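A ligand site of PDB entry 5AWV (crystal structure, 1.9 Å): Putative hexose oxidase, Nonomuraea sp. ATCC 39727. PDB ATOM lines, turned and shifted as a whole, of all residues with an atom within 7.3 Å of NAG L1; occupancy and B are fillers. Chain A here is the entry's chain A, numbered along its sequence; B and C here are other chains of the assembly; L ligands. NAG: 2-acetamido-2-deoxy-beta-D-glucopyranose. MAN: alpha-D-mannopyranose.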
ATOM      1  N   ALA A  50      26.892  17.781   8.422  1.00  0.00           N
ATOM      2  CA  ALA A  50      27.165  18.970   9.200  1.00  0.00           C
ATOM      3  C   ALA A  50      28.642  19.350   9.334  1.00  0.00           C
ATOM      4  O   ALA A  50      28.986  20.565   9.307  1.00  0.00           O
ATOM      5  CB  ALA A  50      26.582  18.843  10.588  1.00  0.00           C
ATOM      6  N   HIS A  91      24.453  14.745  11.232  1.00  0.00           N
ATOM      7  CA  HIS A  91      25.205  15.344  12.293  1.00  0.00           C
ATOM      8  C   HIS A  91      26.333  14.564  12.901  1.00  0.00           C
ATOM      9  O   HIS A  91      27.015  15.037  13.796  1.00  0.00           O
ATOM     10  CB  HIS A  91      24.272  15.861  13.403  1.00  0.00           C
ATOM     11  CG  HIS A  91      23.889  17.283  13.155  1.00  0.00           C
ATOM     12  ND1 HIS A  91      24.607  18.387  13.674  1.00  0.00           N
ATOM     13  CD2 HIS A  91      22.983  17.757  12.268  1.00  0.00           C
ATOM     14  CE1 HIS A  91      24.006  19.480  13.157  1.00  0.00           C
ATOM     15  NE2 HIS A  91      23.075  19.128  12.299  1.00  0.00           N
ATOM     16  N   VAL A 301      34.507  34.793  19.711  1.00  0.00           N
ATOM     17  CA  VAL A 301      34.615  34.826  18.279  1.00  0.00           C
ATOM     18  C   VAL A 301      33.548  35.802  17.713  1.00  0.00           C
ATOM     19  O   VAL A 301      32.339  35.502  17.768  1.00  0.00           O
ATOM     20  CB  VAL A 301      34.419  33.410  17.668  1.00  0.00           C
ATOM     21  CG1 VAL A 301      34.565  33.440  16.142  1.00  0.00           C
ATOM     22  CG2 VAL A 301      35.403  32.407  18.290  1.00  0.00           C
ATOM     23  N   GLY A 303      31.326  37.038  15.194  1.00  0.00           N
ATOM     24  CA  GLY A 303      29.905  36.943  14.819  1.00  0.00           C
ATOM     25  C   GLY A 303      29.292  35.626  15.247  1.00  0.00           C
ATOM     26  O   GLY A 303      28.278  35.202  14.712  1.00  0.00           O
ATOM     27  N   MET A 304      29.906  34.962  16.236  1.00  0.00           N
ATOM     28  CA  MET A 304      29.487  33.619  16.627  1.00  0.00           C
ATOM     29  C   MET A 304      28.823  33.784  18.007  1.00  0.00           C
ATOM     30  O   MET A 304      29.503  33.946  19.037  1.00  0.00           O
ATOM     31  CB  MET A 304      30.713  32.703  16.670  1.00  0.00           C
ATOM     32  CG  MET A 304      30.471  31.242  17.005  1.00  0.00           C
ATOM     33  SD  MET A 304      32.009  30.285  17.312  1.00  0.00           S
ATOM     34  CE  MET A 304      31.341  28.854  18.209  1.00  0.00           C
ATOM     35  N   GLY A 356      16.836  26.693  14.956  1.00  0.00           N
ATOM     36  CA  GLY A 356      17.200  27.336  13.681  1.00  0.00           C
ATOM     37  C   GLY A 356      18.182  26.686  12.719  1.00  0.00           C
ATOM     38  O   GLY A 356      18.917  27.409  12.018  1.00  0.00           O
ATOM     39  N   ARG A 357      18.207  25.347  12.616  1.00  0.00           N
ATOM     40  CA  ARG A 357      19.205  24.655  11.768  1.00  0.00           C
ATOM     41  C   ARG A 357      18.628  23.922  10.570  1.00  0.00           C
ATOM     42  O   ARG A 357      17.562  23.314  10.693  1.00  0.00           O
ATOM     43  CB  ARG A 357      20.024  23.623  12.573  1.00  0.00           C
ATOM     44  CG  ARG A 357      21.394  23.228  11.980  1.00  0.00           C
ATOM     45  CD  ARG A 357      22.510  24.228  12.305  1.00  0.00           C
ATOM     46  NE  ARG A 357      21.983  25.581  12.567  1.00  0.00           N
ATOM     47  CZ  ARG A 357      22.015  26.648  11.736  1.00  0.00           C
ATOM     48  NH1 ARG A 357      22.606  26.606  10.553  1.00  0.00           N
ATOM     49  NH2 ARG A 357      21.454  27.791  12.133  1.00  0.00           N
ATOM     50  N   GLY A 358      19.322  23.928   9.423  1.00  0.00           N
ATOM     51  CA  GLY A 358      20.572  24.686   9.160  1.00  0.00           C
ATOM     52  C   GLY A 358      21.494  24.142   8.067  1.00  0.00           C
ATOM     53  O   GLY A 358      21.478  24.640   6.934  1.00  0.00           O
ATOM     54  N   GLY A 359      22.309  23.141   8.417  1.00  0.00           N
ATOM     55  CA  GLY A 359      23.085  22.383   7.441  1.00  0.00           C
ATOM     56  C   GLY A 359      24.582  22.353   7.667  1.00  0.00           C
ATOM     57  O   GLY A 359      25.021  22.098   8.786  1.00  0.00           O
ATOM     58  N   ARG A 360      25.372  22.605   6.604  1.00  0.00           N
ATOM     59  CA  ARG A 360      26.810  22.328   6.628  1.00  0.00           C
ATOM     60  C   ARG A 360      27.596  23.425   7.325  1.00  0.00           C
ATOM     61  O   ARG A 360      27.524  24.576   6.942  1.00  0.00           O
ATOM     62  CB  ARG A 360      27.356  22.130   5.237  1.00  0.00           C
ATOM     63  CG  ARG A 360      28.795  21.598   5.222  1.00  0.00           C
ATOM     64  CD  ARG A 360      29.124  21.144   3.815  1.00  0.00           C
ATOM     65  NE  ARG A 360      30.329  20.354   3.646  1.00  0.00           N
ATOM     66  CZ  ARG A 360      30.496  19.080   3.961  1.00  0.00           C
ATOM     67  NH1 ARG A 360      29.574  18.396   4.633  1.00  0.00           N
ATOM     68  NH2 ARG A 360      31.656  18.502   3.679  1.00  0.00           N
ATOM     69  N   GLY A 361      28.406  23.039   8.294  1.00  0.00           N
ATOM     70  CA  GLY A 361      29.088  23.985   9.166  1.00  0.00           C
ATOM     71  C   GLY A 361      30.578  23.987   8.969  1.00  0.00           C
ATOM     72  O   GLY A 361      31.084  23.286   8.135  1.00  0.00           O
ATOM     73  N   PRO A 362      31.307  24.761   9.781  1.00  0.00           N
ATOM     74  CA  PRO A 362      32.768  24.737   9.719  1.00  0.00           C
ATOM     75  C   PRO A 362      33.319  23.419  10.258  1.00  0.00           C
ATOM     76  O   PRO A 362      32.602  22.573  10.799  1.00  0.00           O
ATOM     77  CB  PRO A 362      33.162  25.917  10.614  1.00  0.00           C
ATOM     78  CG  PRO A 362      32.118  25.862  11.685  1.00  0.00           C
ATOM     79  CD  PRO A 362      30.836  25.345  11.043  1.00  0.00           C
ATOM     80  N   GHP B   5      22.237  27.682  16.750  1.00  0.00           N
ATOM     81  CA  GHP B   5      22.698  28.872  15.958  1.00  0.00           C
ATOM     82  C   GHP B   5      23.100  28.206  14.785  1.00  0.00           C
ATOM     83  O   GHP B   5      22.427  27.223  14.486  1.00  0.00           O
ATOM     84  C1  GHP B   5      21.756  29.811  15.501  1.00  0.00           C
ATOM     85  C2  GHP B   5      22.256  31.054  15.136  1.00  0.00           C
ATOM     86  C3  GHP B   5      21.446  32.045  14.593  1.00  0.00           C
ATOM     87  C4  GHP B   5      20.067  31.768  14.421  1.00  0.00           C
ATOM     88  O4  GHP B   5      19.261  32.732  13.927  1.00  0.00           O
ATOM     89  C5  GHP B   5      19.543  30.526  14.771  1.00  0.00           C
ATOM     90  C6  GHP B   5      20.386  29.540  15.299  1.00  0.00           C
ATOM     91  N   OMY B   6      24.070  28.489  13.792  1.00  0.00           N
ATOM     92  CA  OMY B   6      25.177  29.471  13.626  1.00  0.00           C
ATOM     93  OCZ OMY B   6      25.975  24.197  16.805  1.00  0.00           O
ATOM     94  CE2 OMY B   6      25.736  25.129  14.581  1.00  0.00           C
ATOM     95  CE1 OMY B   6      26.625  26.525  16.362  1.00  0.00           C
ATOM     96  CZ  OMY B   6      26.117  25.267  15.912  1.00  0.00           C
ATOM     97  CG  OMY B   6      26.386  27.457  14.138  1.00  0.00           C
ATOM     98  CD2 OMY B   6      25.874  26.207  13.709  1.00  0.00           C
ATOM     99  CD1 OMY B   6      26.733  27.602  15.483  1.00  0.00           C
ATOM    100  CB  OMY B   6      26.476  28.620  13.293  1.00  0.00           C
ATOM    101 CL   OMY B   6      27.124  26.832  18.000  1.00  0.00          CL
ATOM    102  O   OMY B   6      24.559  29.853  11.345  1.00  0.00           O
ATOM    103  C   OMY B   6      24.625  30.317  12.623  1.00  0.00           C
ATOM    104  ODE OMY B   6      26.455  28.296  11.888  1.00  0.00           O
ATOM    105  N   3FG B   7      24.074  31.495  12.990  1.00  0.00           N
ATOM    106  OD1 3FG B   7      21.049  33.919  16.306  1.00  0.00           O
ATOM    107  CD1 3FG B   7      21.884  34.290  15.267  1.00  0.00           C
ATOM    108  CG1 3FG B   7      22.099  33.278  14.318  1.00  0.00           C
ATOM    109  CZ  3FG B   7      22.494  35.547  15.163  1.00  0.00           C
ATOM    110  CD2 3FG B   7      23.327  35.804  14.068  1.00  0.00           C
ATOM    111  OD2 3FG B   7      23.911  37.019  13.950  1.00  0.00           O
ATOM    112  CG2 3FG B   7      23.576  34.805  13.115  1.00  0.00           C
ATOM    113  CB  3FG B   7      22.965  33.527  13.207  1.00  0.00           C
ATOM    114  CA  3FG B   7      23.228  32.485  12.229  1.00  0.00           C
ATOM    115  C   3FG B   7      23.679  32.921  10.952  1.00  0.00           C
ATOM    116  O   3FG B   7      22.915  33.698  10.325  1.00  0.00           O
ATOM    117  OXT 3FG B   7      24.757  32.450  10.493  1.00  0.00           O
ATOM    118  N   THR C 354      19.781  25.742   2.304  1.00  0.00           N
ATOM    119  CA  THR C 354      18.364  25.478   2.631  1.00  0.00           C
ATOM    120  C   THR C 354      17.574  26.807   2.669  1.00  0.00           C
ATOM    121  O   THR C 354      18.064  27.791   3.266  1.00  0.00           O
ATOM    122  CB  THR C 354      18.192  24.682   3.951  1.00  0.00           C
ATOM    123  OG1 THR C 354      19.275  24.981   4.841  1.00  0.00           O
ATOM    124  CG2 THR C 354      18.139  23.167   3.680  1.00  0.00           C
HETATM  125  C1  NAG L   1      27.597  28.420  10.988  1.00  0.00           C
HETATM  126  C2  NAG L   1      27.084  27.932   9.647  1.00  0.00           C
HETATM  127  C3  NAG L   1      28.228  27.836   8.638  1.00  0.00           C
HETATM  128  C4  NAG L   1      28.983  29.145   8.513  1.00  0.00           C
HETATM  129  C5  NAG L   1      29.327  29.708   9.892  1.00  0.00           C
HETATM  130  C6  NAG L   1      29.944  31.077   9.696  1.00  0.00           C
HETATM  131  C7  NAG L   1      25.428  26.082   9.237  1.00  0.00           C
HETATM  132  C8  NAG L   1      24.678  26.925   8.165  1.00  0.00           C
HETATM  133  N2  NAG L   1      26.500  26.591   9.872  1.00  0.00           N
HETATM  134  O3  NAG L   1      27.684  27.505   7.356  1.00  0.00           O
HETATM  135  O4  NAG L   1      30.213  28.873   7.813  1.00  0.00           O
HETATM  136  O5  NAG L   1      28.135  29.762  10.758  1.00  0.00           O
HETATM  137  O6  NAG L   1      30.636  31.269  10.929  1.00  0.00           O
HETATM  138  O7  NAG L   1      25.000  24.971   9.524  1.00  0.00           O
HETATM  139  C1  MAN L   2      22.917  35.463   5.697  1.00  0.00           C
HETATM  140  C2  MAN L   2      22.502  34.740   4.419  1.00  0.00           C
HETATM  141  C3  MAN L   2      22.394  33.245   4.636  1.00  0.00           C
HETATM  142  C4  MAN L   2      23.711  32.721   5.140  1.00  0.00           C
HETATM  143  C5  MAN L   2      24.081  33.446   6.438  1.00  0.00           C
HETATM  144  C6  MAN L   2      25.399  32.886   6.954  1.00  0.00           C
HETATM  145  O2  MAN L   2      23.462  35.030   3.374  1.00  0.00           O
HETATM  146  O3  MAN L   2      22.090  32.597   3.410  1.00  0.00           O
HETATM  147  O4  MAN L   2      23.543  31.334   5.366  1.00  0.00           O
HETATM  148  O5  MAN L   2      24.162  34.877   6.195  1.00  0.00           O
HETATM  149  O6  MAN L   2      25.994  33.919   7.750  1.00  0.00           O
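N of Gly 361 is in hydrogen-bond range of O of Ala 50. O of Gly 358 sits at hydrogen-bond distance from OG1 of Thr 354 of chain C, at 3.1 Å. O of GHP 5 of chain B is in hydrogen-bond range of the guanidinium group of Arg 357 (2.6 Å).
OXT of 3FG 7 of chain B lies within hydrogen-bond range of O6 of MAN L2, 3.3 Å away. ODE of OMY 6 of chain B is covalently linked to a carbon (C1) of NAG L1 (1.5 Å). The guanidinium group (NH1) of Arg 357 lies within hydrogen-bond range of an oxygen (O7) of NAG L1, 3.1 Å away. The backbone carbonyl oxygen (O) of Arg 360 sits at hydrogen-bond distance from an oxygen (O3) of NAG L1 (3.0 Å). N of Gly 359 sits close to O7 of NAG L1 (3.4 Å).
Residues that only touch NAG L1: Gly 361 (3.7 Å) and Gly 358 (3.9 Å).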
